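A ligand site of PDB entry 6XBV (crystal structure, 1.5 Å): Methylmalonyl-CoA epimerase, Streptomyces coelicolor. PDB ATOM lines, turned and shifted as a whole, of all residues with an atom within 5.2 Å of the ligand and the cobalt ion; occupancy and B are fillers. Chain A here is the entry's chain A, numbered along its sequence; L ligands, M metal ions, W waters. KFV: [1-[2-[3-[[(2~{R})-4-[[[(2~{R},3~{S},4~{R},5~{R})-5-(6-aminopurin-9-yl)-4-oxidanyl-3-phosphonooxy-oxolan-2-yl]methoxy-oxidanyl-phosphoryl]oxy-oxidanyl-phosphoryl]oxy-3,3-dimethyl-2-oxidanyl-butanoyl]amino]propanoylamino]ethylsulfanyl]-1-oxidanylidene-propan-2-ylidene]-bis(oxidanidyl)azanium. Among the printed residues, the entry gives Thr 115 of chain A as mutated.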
ATOM      1  N   HIS A   7      13.280  27.958  19.476  1.00  0.00           N
ATOM      2  CA  HIS A   7      12.623  26.757  20.026  1.00  0.00           C
ATOM      3  C   HIS A   7      13.121  26.525  21.441  1.00  0.00           C
ATOM      4  O   HIS A   7      14.177  27.016  21.871  1.00  0.00           O
ATOM      5  CB  HIS A   7      12.756  25.526  19.161  1.00  0.00           C
ATOM      6  CG  HIS A   7      14.166  25.047  18.891  1.00  0.00           C
ATOM      7  ND1 HIS A   7      14.897  25.502  17.756  1.00  0.00           N
ATOM      8  CD2 HIS A   7      14.907  24.084  19.501  1.00  0.00           C
ATOM      9  CE1 HIS A   7      16.026  24.770  17.767  1.00  0.00           C
ATOM     10  NE2 HIS A   7      16.102  23.918  18.807  1.00  0.00           N
ATOM     11  N   ASN A  36      18.123  12.841  13.324  1.00  0.00           N
ATOM     12  CA  ASN A  36      19.435  13.461  13.075  1.00  0.00           C
ATOM     13  C   ASN A  36      20.452  12.480  13.618  1.00  0.00           C
ATOM     14  O   ASN A  36      20.626  12.416  14.844  1.00  0.00           O
ATOM     15  CB  ASN A  36      19.555  14.866  13.680  1.00  0.00           C
ATOM     16  CG  ASN A  36      20.811  15.580  13.246  1.00  0.00           C
ATOM     17  OD1 ASN A  36      21.886  14.997  13.329  1.00  0.00           O
ATOM     18  ND2 ASN A  36      20.691  16.876  12.922  1.00  0.00           N
ATOM     19  N   GLN A  39      23.588  13.975  15.546  1.00  0.00           N
ATOM     20  CA  GLN A  39      23.279  14.477  16.904  1.00  0.00           C
ATOM     21  C   GLN A  39      22.734  13.363  17.774  1.00  0.00           C
ATOM     22  O   GLN A  39      22.786  13.523  18.984  1.00  0.00           O
ATOM     23  CB  GLN A  39      22.288  15.654  16.833  1.00  0.00           C
ATOM     24  CG  GLN A  39      22.878  16.887  16.198  1.00  0.00           C
ATOM     25  CD  GLN A  39      23.928  17.587  17.027  1.00  0.00           C
ATOM     26  OE1 GLN A  39      24.094  17.317  18.233  1.00  0.00           O
ATOM     27  NE2 GLN A  39      24.730  18.412  16.344  1.00  0.00           N
ATOM     28  N   VAL A  41      19.451  12.010  17.755  1.00  0.00           N
ATOM     29  CA  VAL A  41      18.063  12.327  18.213  1.00  0.00           C
ATOM     30  C   VAL A  41      17.042  11.940  17.140  1.00  0.00           C
ATOM     31  O   VAL A  41      17.303  12.121  15.927  1.00  0.00           O
ATOM     32  CB  VAL A  41      17.874  13.813  18.564  1.00  0.00           C
ATOM     33  CG1 VAL A  41      18.710  14.197  19.775  1.00  0.00           C
ATOM     34  CG2 VAL A  41      18.169  14.757  17.409  1.00  0.00           C
ATOM     35  N   GLU A  43      13.361  13.635  16.517  1.00  0.00           N
ATOM     36  CA  GLU A  43      12.737  14.879  17.026  1.00  0.00           C
ATOM     37  C   GLU A  43      11.419  15.157  16.377  1.00  0.00           C
ATOM     38  O   GLU A  43      11.116  14.725  15.212  1.00  0.00           O
ATOM     39  CB  GLU A  43      13.702  16.025  16.910  1.00  0.00           C
ATOM     40  CG  GLU A  43      14.132  16.250  15.524  1.00  0.00           C
ATOM     41  CD  GLU A  43      14.545  17.682  15.230  1.00  0.00           C
ATOM     42  OE1 GLU A  43      15.679  17.865  14.729  1.00  0.00           O
ATOM     43  OE2 GLU A  43      13.699  18.607  15.461  1.00  0.00           O
ATOM     44  N   GLN A  60      10.696  21.724  20.482  1.00  0.00           N
ATOM     45  CA  GLN A  60      11.461  20.644  19.840  1.00  0.00           C
ATOM     46  C   GLN A  60      11.536  19.504  20.835  1.00  0.00           C
ATOM     47  O   GLN A  60      12.315  19.573  21.813  1.00  0.00           O
ATOM     48  CB  GLN A  60      12.824  21.160  19.424  1.00  0.00           C
ATOM     49  CG  GLN A  60      13.698  20.082  18.818  1.00  0.00           C
ATOM     50  CD  GLN A  60      15.034  20.613  18.391  1.00  0.00           C
ATOM     51  OE1 GLN A  60      15.810  20.986  19.242  1.00  0.00           O
ATOM     52  NE2 GLN A  60      15.213  20.733  17.083  1.00  0.00           N
ATOM     53  N   LEU A  62      12.668  15.751  21.820  1.00  0.00           N
ATOM     54  CA  LEU A  62      13.831  14.950  21.391  1.00  0.00           C
ATOM     55  C   LEU A  62      13.863  13.677  22.190  1.00  0.00           C
ATOM     56  O   LEU A  62      13.989  13.723  23.420  1.00  0.00           O
ATOM     57  CB  LEU A  62      15.137  15.746  21.596  1.00  0.00           C
ATOM     58  CG  LEU A  62      15.184  17.106  20.908  1.00  0.00           C
ATOM     59  CD1 LEU A  62      15.477  18.121  21.956  1.00  0.00           C
ATOM     60  CD2 LEU A  62      16.183  17.154  19.785  1.00  0.00           C
ATOM     61  N   ALA A  70      24.376  13.221  23.267  1.00  0.00           N
ATOM     62  CA  ALA A  70      24.103  14.337  24.192  1.00  0.00           C
ATOM     63  C   ALA A  70      22.800  14.106  24.969  1.00  0.00           C
ATOM     64  O   ALA A  70      22.735  14.269  26.194  1.00  0.00           O
ATOM     65  CB  ALA A  70      24.112  15.640  23.446  1.00  0.00           C
ATOM     66  N   VAL A  71      21.711  13.813  24.264  1.00  0.00           N
ATOM     67  CA  VAL A  71      20.393  13.674  24.922  1.00  0.00           C
ATOM     68  C   VAL A  71      20.337  12.362  25.701  1.00  0.00           C
ATOM     69  O   VAL A  71      19.719  12.369  26.797  1.00  0.00           O
ATOM     70  CB  VAL A  71      19.252  13.830  23.905  1.00  0.00           C
ATOM     71  CG1 VAL A  71      17.933  13.569  24.561  1.00  0.00           C
ATOM     72  CG2 VAL A  71      19.275  15.251  23.307  1.00  0.00           C
ATOM     73  N   LYS A  73      22.744  10.811  27.311  1.00  0.00           N
ATOM     74  CA  LYS A  73      23.527  11.013  28.552  1.00  0.00           C
ATOM     75  C   LYS A  73      22.740  11.923  29.488  1.00  0.00           C
ATOM     76  O   LYS A  73      22.669  11.700  30.730  1.00  0.00           O
ATOM     77  CB  LYS A  73      24.874  11.672  28.295  1.00  0.00           C
ATOM     78  CG  LYS A  73      25.969  10.784  27.726  1.00  0.00           C
ATOM     79  CD  LYS A  73      27.318  11.499  27.717  1.00  0.00           C
ATOM     80  CE  LYS A  73      27.637  12.172  29.033  1.00  0.00           C
ATOM     81  NZ  LYS A  73      29.095  12.430  29.208  1.00  0.00           N
ATOM     82  N   TRP A  74      22.191  12.995  28.946  1.00  0.00           N
ATOM     83  CA  TRP A  74      21.469  13.952  29.767  1.00  0.00           C
ATOM     84  C   TRP A  74      20.254  13.309  30.426  1.00  0.00           C
ATOM     85  O   TRP A  74      19.982  13.556  31.617  1.00  0.00           O
ATOM     86  CB  TRP A  74      21.144  15.168  28.884  1.00  0.00           C
ATOM     87  CG  TRP A  74      20.687  16.306  29.695  1.00  0.00           C
ATOM     88  CD1 TRP A  74      21.444  17.286  30.248  1.00  0.00           C
ATOM     89  CD2 TRP A  74      19.342  16.584  30.028  1.00  0.00           C
ATOM     90  NE1 TRP A  74      20.661  18.131  30.945  1.00  0.00           N
ATOM     91  CE2 TRP A  74      19.359  17.746  30.819  1.00  0.00           C
ATOM     92  CE3 TRP A  74      18.133  15.960  29.746  1.00  0.00           C
ATOM     93  CZ2 TRP A  74      18.204  18.312  31.318  1.00  0.00           C
ATOM     94  CZ3 TRP A  74      16.993  16.498  30.242  1.00  0.00           C
ATOM     95  CH2 TRP A  74      17.022  17.644  31.010  1.00  0.00           C
ATOM     96  N   LYS A  77      21.166  11.080  33.409  1.00  0.00           N
ATOM     97  CA  LYS A  77      21.571  11.853  34.602  1.00  0.00           C
ATOM     98  C   LYS A  77      20.377  12.599  35.202  1.00  0.00           C
ATOM     99  O   LYS A  77      20.316  12.691  36.424  1.00  0.00           O
ATOM    100  CB  LYS A  77      22.680  12.893  34.374  1.00  0.00           C
ATOM    101  CG  LYS A  77      22.898  13.847  35.565  1.00  0.00           C
ATOM    102  CD  LYS A  77      23.809  15.055  35.361  1.00  0.00           C
ATOM    103  CE  LYS A  77      23.897  15.968  36.566  1.00  0.00           C
ATOM    104  NZ  LYS A  77      22.918  17.097  36.530  1.00  0.00           N
ATOM    105  N   HIS A  83      16.085  20.604  27.958  1.00  0.00           N
ATOM    106  CA  HIS A  83      17.475  20.301  27.626  1.00  0.00           C
ATOM    107  C   HIS A  83      18.242  21.505  27.102  1.00  0.00           C
ATOM    108  O   HIS A  83      19.399  21.690  27.437  1.00  0.00           O
ATOM    109  CB  HIS A  83      17.454  19.157  26.612  1.00  0.00           C
ATOM    110  CG  HIS A  83      18.810  18.774  26.105  1.00  0.00           C
ATOM    111  ND1 HIS A  83      19.324  19.196  24.902  1.00  0.00           N
ATOM    112  CD2 HIS A  83      19.828  18.052  26.698  1.00  0.00           C
ATOM    113  CE1 HIS A  83      20.594  18.765  24.785  1.00  0.00           C
ATOM    114  NE2 HIS A  83      20.882  18.032  25.848  1.00  0.00           N
ATOM    115  N   HIS A  84      17.602  22.362  26.281  1.00  0.00           N
ATOM    116  CA  HIS A  84      18.331  23.509  25.700  1.00  0.00           C
ATOM    117  C   HIS A  84      17.348  24.584  25.282  1.00  0.00           C
ATOM    118  O   HIS A  84      16.141  24.261  25.171  1.00  0.00           O
ATOM    119  CB  HIS A  84      19.273  23.145  24.562  1.00  0.00           C
ATOM    120  CG  HIS A  84      18.620  22.635  23.322  1.00  0.00           C
ATOM    121  ND1 HIS A  84      18.400  21.271  23.122  1.00  0.00           N
ATOM    122  CD2 HIS A  84      18.311  23.257  22.143  1.00  0.00           C
ATOM    123  CE1 HIS A  84      17.903  21.122  21.870  1.00  0.00           C
ATOM    124  NE2 HIS A  84      17.851  22.308  21.227  1.00  0.00           N
ATOM    125  N   ALA A  86      16.990  27.692  22.094  1.00  0.00           N
ATOM    126  CA  ALA A  86      17.574  28.090  20.814  1.00  0.00           C
ATOM    127  C   ALA A  86      17.107  29.493  20.430  1.00  0.00           C
ATOM    128  O   ALA A  86      15.868  29.750  20.446  1.00  0.00           O
ATOM    129  CB  ALA A  86      17.189  27.094  19.746  1.00  0.00           C
ATOM    130  N   LEU A 107      30.789  25.478  20.476  1.00  0.00           N
ATOM    131  CA  LEU A 107      31.168  24.064  20.403  1.00  0.00           C
ATOM    132  C   LEU A 107      31.584  23.686  18.961  1.00  0.00           C
ATOM    133  O   LEU A 107      32.425  22.767  18.854  1.00  0.00           O
ATOM    134  CB  LEU A 107      30.009  23.188  20.861  1.00  0.00           C
ATOM    135  CG  LEU A 107      29.501  23.342  22.268  1.00  0.00           C
ATOM    136  CD1 LEU A 107      28.578  22.178  22.581  1.00  0.00           C
ATOM    137  CD2 LEU A 107      30.557  23.481  23.330  1.00  0.00           C
ATOM    138  N   TYR A 108      31.113  24.301  17.912  1.00  0.00           N
ATOM    139  CA  TYR A 108      31.501  23.859  16.535  1.00  0.00           C
ATOM    140  C   TYR A 108      32.370  24.926  15.857  1.00  0.00           C
ATOM    141  O   TYR A 108      32.103  26.087  15.979  1.00  0.00           O
ATOM    142  CB  TYR A 108      30.227  23.524  15.744  1.00  0.00           C
ATOM    143  CG  TYR A 108      29.316  22.516  16.398  1.00  0.00           C
ATOM    144  CD1 TYR A 108      29.776  21.473  17.137  1.00  0.00           C
ATOM    145  CD2 TYR A 108      27.947  22.542  16.166  1.00  0.00           C
ATOM    146  CE1 TYR A 108      28.948  20.544  17.746  1.00  0.00           C
ATOM    147  CE2 TYR A 108      27.096  21.648  16.767  1.00  0.00           C
ATOM    148  CZ  TYR A 108      27.575  20.625  17.565  1.00  0.00           C
ATOM    149  OH  TYR A 108      26.740  19.763  18.196  1.00  0.00           O
ATOM    150  N   ARG A 113      24.412  20.810  10.485  1.00  0.00           N
ATOM    151  CA  ARG A 113      22.990  20.661  10.038  1.00  0.00           C
ATOM    152  C   ARG A 113      22.088  20.358  11.218  1.00  0.00           C
ATOM    153  O   ARG A 113      22.337  19.437  12.033  1.00  0.00           O
ATOM    154  CB  ARG A 113      22.837  19.471   9.068  1.00  0.00           C
ATOM    155  CG  ARG A 113      21.395  19.253   8.635  1.00  0.00           C
ATOM    156  CD  ARG A 113      21.188  18.527   7.304  1.00  0.00           C
ATOM    157  NE  ARG A 113      21.654  17.146   7.405  1.00  0.00           N
ATOM    158  CZ  ARG A 113      20.998  16.142   7.982  1.00  0.00           C
ATOM    159  NH1 ARG A 113      19.800  16.325   8.504  1.00  0.00           N
ATOM    160  NH2 ARG A 113      21.543  14.929   7.982  1.00  0.00           N
ATOM    161  N   GLY A 114      20.996  21.100  11.286  1.00  0.00           N
ATOM    162  CA  GLY A 114      19.930  20.844  12.257  1.00  0.00           C
ATOM    163  C   GLY A 114      18.613  20.625  11.523  1.00  0.00           C
ATOM    164  O   GLY A 114      18.586  20.420  10.256  1.00  0.00           O
ATOM    165  N   THR A 115      17.531  20.860  12.205  1.00  0.00           N
ATOM    166  CA  THR A 115      16.148  20.527  11.800  1.00  0.00           C
ATOM    167  C   THR A 115      15.777  21.218  10.491  1.00  0.00           C
ATOM    168  O   THR A 115      16.035  22.422  10.398  1.00  0.00           O
ATOM    169  CB  THR A 115      15.244  21.041  12.920  1.00  0.00           C
ATOM    170  OG1 THR A 115      15.837  20.560  14.116  1.00  0.00           O
ATOM    171  CG2 THR A 115      13.818  20.591  12.743  1.00  0.00           C
ATOM    172  N   SER A 118      18.222  23.487   8.725  1.00  0.00           N
ATOM    173  CA  SER A 118      18.766  24.675   9.432  1.00  0.00           C
ATOM    174  C   SER A 118      20.271  24.456   9.636  1.00  0.00           C
ATOM    175  O   SER A 118      20.783  23.314   9.593  1.00  0.00           O
ATOM    176  CB  SER A 118      18.049  24.942  10.768  1.00  0.00           C
ATOM    177  OG  SER A 118      18.150  23.880  11.659  1.00  0.00           O
ATOM    178  N   ILE A 120      23.189  25.186  12.630  1.00  0.00           N
ATOM    179  CA  ILE A 120      23.090  25.379  14.113  1.00  0.00           C
ATOM    180  C   ILE A 120      24.482  25.384  14.703  1.00  0.00           C
ATOM    181  O   ILE A 120      25.401  24.701  14.200  1.00  0.00           O
ATOM    182  CB  ILE A 120      22.232  24.293  14.779  1.00  0.00           C
ATOM    183  CG1 ILE A 120      22.867  22.897  14.757  1.00  0.00           C
ATOM    184  CG2 ILE A 120      20.834  24.283  14.135  1.00  0.00           C
ATOM    185  CD1 ILE A 120      22.077  21.826  15.487  1.00  0.00           C
ATOM    186  N   PHE A 122      26.205  25.594  19.082  1.00  0.00           N
ATOM    187  CA  PHE A 122      25.858  25.597  20.514  1.00  0.00           C
ATOM    188  C   PHE A 122      26.919  26.340  21.311  1.00  0.00           C
ATOM    189  O   PHE A 122      28.101  26.333  20.883  1.00  0.00           O
ATOM    190  CB  PHE A 122      25.720  24.212  21.102  1.00  0.00           C
ATOM    191  CG  PHE A 122      24.538  23.413  20.606  1.00  0.00           C
ATOM    192  CD1 PHE A 122      23.320  23.464  21.253  1.00  0.00           C
ATOM    193  CD2 PHE A 122      24.703  22.589  19.494  1.00  0.00           C
ATOM    194  CE1 PHE A 122      22.235  22.715  20.759  1.00  0.00           C
ATOM    195  CE2 PHE A 122      23.629  21.867  19.017  1.00  0.00           C
ATOM    196  CZ  PHE A 122      22.426  21.904  19.665  1.00  0.00           C
ATOM    197  N   HIS A 124      28.578  26.566  25.252  1.00  0.00           N
ATOM    198  CA  HIS A 124      28.734  25.651  26.395  1.00  0.00           C
ATOM    199  C   HIS A 124      27.913  26.136  27.594  1.00  0.00           C
ATOM    200  O   HIS A 124      27.992  27.319  27.976  1.00  0.00           O
ATOM    201  CB  HIS A 124      30.242  25.567  26.769  1.00  0.00           C
ATOM    202  CG  HIS A 124      30.533  24.374  27.590  1.00  0.00           C
ATOM    203  ND1 HIS A 124      30.011  24.183  28.867  1.00  0.00           N
ATOM    204  CD2 HIS A 124      31.256  23.251  27.283  1.00  0.00           C
ATOM    205  CE1 HIS A 124      30.470  22.981  29.329  1.00  0.00           C
ATOM    206  NE2 HIS A 124      31.170  22.426  28.387  1.00  0.00           N
ATOM    207  N   PRO A 125      27.081  25.248  28.210  1.00  0.00           N
ATOM    208  CA  PRO A 125      26.262  25.678  29.316  1.00  0.00           C
ATOM    209  C   PRO A 125      27.008  26.234  30.496  1.00  0.00           C
ATOM    210  O   PRO A 125      26.501  27.121  31.200  1.00  0.00           O
ATOM    211  CB  PRO A 125      25.481  24.417  29.672  1.00  0.00           C
ATOM    212  CG  PRO A 125      26.336  23.269  29.163  1.00  0.00           C
ATOM    213  CD  PRO A 125      26.933  23.833  27.886  1.00  0.00           C
ATOM    214  N   LYS A 126      28.253  25.750  30.705  1.00  0.00           N
ATOM    215  CA  LYS A 126      28.974  26.308  31.861  1.00  0.00           C
ATOM    216  C   LYS A 126      29.431  27.728  31.612  1.00  0.00           C
ATOM    217  O   LYS A 126      29.833  28.397  32.620  1.00  0.00           O
ATOM    218  CB  LYS A 126      30.197  25.404  32.109  1.00  0.00           C
ATOM    219  CG  LYS A 126      29.827  24.031  32.616  1.00  0.00           C
ATOM    220  CD  LYS A 126      29.166  24.013  33.957  1.00  0.00           C
ATOM    221  CE  LYS A 126      30.118  24.503  35.030  1.00  0.00           C
ATOM    222  NZ  LYS A 126      31.470  23.877  34.949  1.00  0.00           N
ATOM    223  N   GLY A 130      24.484  27.922  33.101  1.00  0.00           N
ATOM    224  CA  GLY A 130      23.813  26.627  33.209  1.00  0.00           C
ATOM    225  C   GLY A 130      22.832  26.302  32.091  1.00  0.00           C
ATOM    226  O   GLY A 130      22.132  25.321  32.245  1.00  0.00           O
ATOM    227  N   VAL A 131      22.760  27.174  31.066  1.00  0.00           N
ATOM    228  CA  VAL A 131      21.761  26.964  29.978  1.00  0.00           C
ATOM    229  C   VAL A 131      22.483  26.581  28.692  1.00  0.00           C
ATOM    230  O   VAL A 131      23.281  27.366  28.144  1.00  0.00           O
ATOM    231  CB  VAL A 131      20.895  28.226  29.767  1.00  0.00           C
ATOM    232  CG1 VAL A 131      19.941  27.979  28.586  1.00  0.00           C
ATOM    233  CG2 VAL A 131      20.158  28.548  31.029  1.00  0.00           C
ATOM    234  N   LEU A 132      22.271  25.339  28.218  1.00  0.00           N
ATOM    235  CA  LEU A 132      22.778  24.954  26.890  1.00  0.00           C
ATOM    236  C   LEU A 132      22.045  25.832  25.874  1.00  0.00           C
ATOM    237  O   LEU A 132      20.816  25.724  25.801  1.00  0.00           O
ATOM    238  CB  LEU A 132      22.635  23.451  26.654  1.00  0.00           C
ATOM    239  CG  LEU A 132      23.035  22.978  25.253  1.00  0.00           C
ATOM    240  CD1 LEU A 132      24.512  23.198  24.889  1.00  0.00           C
ATOM    241  CD2 LEU A 132      22.714  21.496  25.149  1.00  0.00           C
ATOM    242  N   GLU A 134      21.551  27.186  21.971  1.00  0.00           N
ATOM    243  CA  GLU A 134      21.691  26.963  20.509  1.00  0.00           C
ATOM    244  C   GLU A 134      21.492  28.258  19.762  1.00  0.00           C
ATOM    245  O   GLU A 134      20.601  29.067  20.139  1.00  0.00           O
ATOM    246  CB  GLU A 134      20.691  25.901  20.070  1.00  0.00           C
ATOM    247  CG  GLU A 134      20.797  25.458  18.622  1.00  0.00           C
ATOM    248  CD  GLU A 134      19.708  24.506  18.171  1.00  0.00           C
ATOM    249  OE1 GLU A 134      19.201  23.785  18.999  1.00  0.00           O
ATOM    250  OE2 GLU A 134      19.221  24.745  16.965  1.00  0.00           O
HETATM  251  N1  KFV L   1      22.202  21.847  30.048  1.00  0.00           N
HETATM  252  C2  KFV L   1      22.930  22.310  31.094  1.00  0.00           C
HETATM  253  N3  KFV L   1      24.066  21.834  31.494  1.00  0.00           N
HETATM  254  C4  KFV L   1      24.495  20.718  30.910  1.00  0.00           C
HETATM  255  C5  KFV L   1      23.804  20.117  29.801  1.00  0.00           C
HETATM  256  C6  KFV L   1      22.531  20.711  29.373  1.00  0.00           C
HETATM  257  N6  KFV L   1      21.816  20.232  28.336  1.00  0.00           N
HETATM  258  N7  KFV L   1      24.443  18.993  29.348  1.00  0.00           N
HETATM  259  C8  KFV L   1      25.548  18.953  30.188  1.00  0.00           C
HETATM  260  N9  KFV L   1      25.590  19.928  31.069  1.00  0.00           N
HETATM  261  C1' KFV L   1      26.635  20.161  32.127  1.00  0.00           C
HETATM  262  C2' KFV L   1      26.829  18.889  32.990  1.00  0.00           C
HETATM  263  O2' KFV L   1      25.882  18.797  34.020  1.00  0.00           O
HETATM  264  C3' KFV L   1      28.255  19.040  33.501  1.00  0.00           C
HETATM  265  O3' KFV L   1      28.146  20.007  34.524  1.00  0.00           O
HETATM  266  C4' KFV L   1      28.932  19.648  32.295  1.00  0.00           C
HETATM  267  O4' KFV L   1      27.868  20.249  31.477  1.00  0.00           O
HETATM  268  C5' KFV L   1      29.565  18.636  31.421  1.00  0.00           C
HETATM  269  O5' KFV L   1      28.651  17.555  31.320  1.00  0.00           O
HETATM  270  O31 KFV L   1      27.941  18.340  36.448  1.00  0.00           O
HETATM  271  P3  KFV L   1      28.716  19.551  36.009  1.00  0.00           P
HETATM  272  O32 KFV L   1      30.141  19.090  35.682  1.00  0.00           O
HETATM  273  O33 KFV L   1      28.446  20.811  36.819  1.00  0.00           O
HETATM  274  P1  KFV L   1      28.906  16.141  30.602  1.00  0.00           P
HETATM  275  O11 KFV L   1      30.287  15.730  31.019  1.00  0.00           O
HETATM  276  O12 KFV L   1      27.761  15.293  31.149  1.00  0.00           O
HETATM  277  O6  KFV L   1      28.732  15.958  29.030  1.00  0.00           O
HETATM  278  P2  KFV L   1      29.713  16.724  28.032  1.00  0.00           P
HETATM  279  O21 KFV L   1      30.597  17.692  28.745  1.00  0.00           O
HETATM  280  O22 KFV L   1      30.560  15.865  27.115  1.00  0.00           O
HETATM  281  O7  KFV L   1      28.611  17.408  27.060  1.00  0.00           O
HETATM  282  CPB KFV L   1      28.072  18.678  27.380  1.00  0.00           C
HETATM  283  CPA KFV L   1      27.778  19.276  26.024  1.00  0.00           C
HETATM  284  CP9 KFV L   1      27.651  20.755  25.919  1.00  0.00           C
HETATM  285  CP8 KFV L   1      29.206  19.310  25.473  1.00  0.00           C
HETATM  286  CP7 KFV L   1      27.284  18.367  24.987  1.00  0.00           C
HETATM  287  OP3 KFV L   1      26.096  17.807  25.440  1.00  0.00           O
HETATM  288  CP6 KFV L   1      26.946  18.930  23.689  1.00  0.00           C
HETATM  289  OP2 KFV L   1      27.802  18.882  22.836  1.00  0.00           O
HETATM  290  NP2 KFV L   1      25.772  19.528  23.359  1.00  0.00           N
HETATM  291  CP5 KFV L   1      25.486  20.028  22.026  1.00  0.00           C
HETATM  292  CP4 KFV L   1      24.765  19.056  21.088  1.00  0.00           C
HETATM  293  CP3 KFV L   1      23.367  18.681  21.505  1.00  0.00           C
HETATM  294  OP1 KFV L   1      22.977  18.976  22.658  1.00  0.00           O
HETATM  295  NP1 KFV L   1      22.689  17.904  20.694  1.00  0.00           N
HETATM  296  CP2 KFV L   1      21.349  17.434  20.947  1.00  0.00           C
HETATM  297  CP1 KFV L   1      20.342  18.501  20.401  1.00  0.00           C
HETATM  298  S   KFV L   1      20.224  18.359  18.588  1.00  0.00           S
HETATM  299  CS1 KFV L   1      19.282  19.724  18.139  1.00  0.00           C
HETATM  300  OS1 KFV L   1      18.875  20.556  18.950  1.00  0.00           O
HETATM  301  CS2 KFV L   1      19.055  19.916  16.746  1.00  0.00           C
HETATM  302  CS3 KFV L   1      19.359  18.791  15.761  1.00  0.00           C
HETATM  303  NS4 KFV L   1      18.375  21.050  16.249  1.00  0.00           N
HETATM  304  OS4 KFV L   1      17.876  22.022  16.919  1.00  0.00           O
HETATM  305  OS5 KFV L   1      18.328  21.095  14.945  1.00  0.00           O
HETATM  306 CO    CO M   1      17.620  22.366  19.056  1.00  0.00          CO
HETATM  307  O   HOH W   1      31.137  16.935  34.188  1.00  0.00           O
HETATM  308  O   HOH W   2      24.033  16.671  32.814  1.00  0.00           O
HETATM  309  O   HOH W   3      31.026  15.791  24.494  1.00  0.00           O
HETATM  310  O   HOH W   4      24.869  15.263  30.586  1.00  0.00           O
HETATM  311  O   HOH W   5      27.997  18.318  20.175  1.00  0.00           O
HETATM  312  O   HOH W   6      17.370  23.879  14.529  1.00  0.00           O
HETATM  313  O   HOH W   7      32.621  19.875  25.484  1.00  0.00           O
HETATM  314  O   HOH W   8      24.935  15.292  27.507  1.00  0.00           O
HETATM  315  O   HOH W   9      32.033  20.937  31.557  1.00  0.00           O
HETATM  316  O   HOH W  10      23.584  17.800  26.941  1.00  0.00           O
HETATM  317  O   HOH W  11      20.212  23.705  29.461  1.00  0.00           O
HETATM  318  O   HOH W  12      28.268  24.165  37.364  1.00  0.00           O
HETATM  319  O   HOH W  13      32.148  19.676  28.422  1.00  0.00           O
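N of Thr 115 is in hydrogen-bond range of OS5 of the ligand, 2.9 Å away.
The side-chain hydroxyl (OG1) of Thr 115 is in hydrogen-bond range of an oxygen (OS5) of the ligand, 2.7 Å away.
OE1 of Gln 39 sits at hydrogen-bond distance from NP1 of the ligand (2.9 Å).
O of His 83 sits at hydrogen-bond distance from N6 of the ligand, at 3.0 Å.
NE2 of His 83 sits close to N6 of the ligand.
An oxygen (O12) of the ligand is in salt-bridge range of the side-chain amino group (NZ) of Lys 73 (3.7 Å).
A ring nitrogen (ND1) of His 83 sits at hydrogen-bond distance from a ring nitrogen (ND1) of His 84 (2.9 Å).
OG1 of Thr 115 sits at hydrogen-bond distance from NE2 of Gln 60 (3.0 Å).
The side-chain carboxylate (OE2) of Glu 43 lies within hydrogen-bond range of the side-chain amide nitrogen (NE2) of Gln 60 (3.1 Å).
OE1 of Glu 43 sits at hydrogen-bond distance from OG1 of Thr 115, 2.8 Å away.
O of Thr 115 lies within hydrogen-bond range of OG of Ser 118 (2.9 Å).
The backbone carbonyl oxygen (O) of Pro 125 lies within hydrogen-bond range of the backbone NH (N) of Gly 130 (2.9 Å).
N of Leu 107 sits at hydrogen-bond distance from O of Phe 122 (2.8 Å).
The side-chain amide nitrogen (ND2) of Asn 36 lies within hydrogen-bond range of the backbone carbonyl oxygen (O) of Arg 113, at 3.2 Å.
Residues that only touch the ligand: Gly 114 (3.1 Å), Gly 130 (3.3 Å), Leu 107 (3.4 Å), Pro 125 (3.5 Å), Trp 74 (3.5 Å), Leu 132 (3.5 Å), Ala 70 (3.6 Å), Tyr 108 (3.6 Å), Phe 122 (3.7 Å), Asn 36 (3.7 Å), Ile 120 (3.8 Å), Val 71 (3.8 Å) and Glu 43 (3.9 Å).
Of the 30 residues printed, 21 come within 4 Å of the ligand.
Along chain A the residues within 4 Å of the ligand span positions 7 to 134.
The cobalt ion is bound by OE1 of Glu 134 (2.1 Å), OS4 of the ligand (2.2 Å), NE2 of His 84 (2.2 Å), NE2 of His 7 (2.2 Å), OS1 of the ligand (2.2 Å) and OE1 of Gln 60 (2.3 Å).
The cobalt ion has six donor atoms within binding distance.
Water W13 lies within hydrogen-bond range of O21 of the ligand (2.5 Å) and NE2 of His 124 (2.9 Å).
Water W5 bridges OP2 of the ligand and OH of Tyr 108.
Water W11 lies within hydrogen-bond range of a nitrogen (N1) of the ligand (2.8 Å), the backbone NH (N) of Leu 132 (2.9 Å) and the backbone carbonyl oxygen (O) of His 83 (3.0 Å).
Water W10 bridges N7 of the ligand (2.8 Å) and NE2 of His 83 (2.9 Å).
Water W6 lies within hydrogen-bond range of OS5 of the ligand (3.0 Å), OG of Ser 118 (3.0 Å) and OE2 of Glu 134 (3.2 Å).
Water W8 lies within hydrogen-bond range of the backbone carbonyl oxygen of Ala 70 (2.8 Å) and an oxygen (OP3) of the ligand (3.5 Å).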
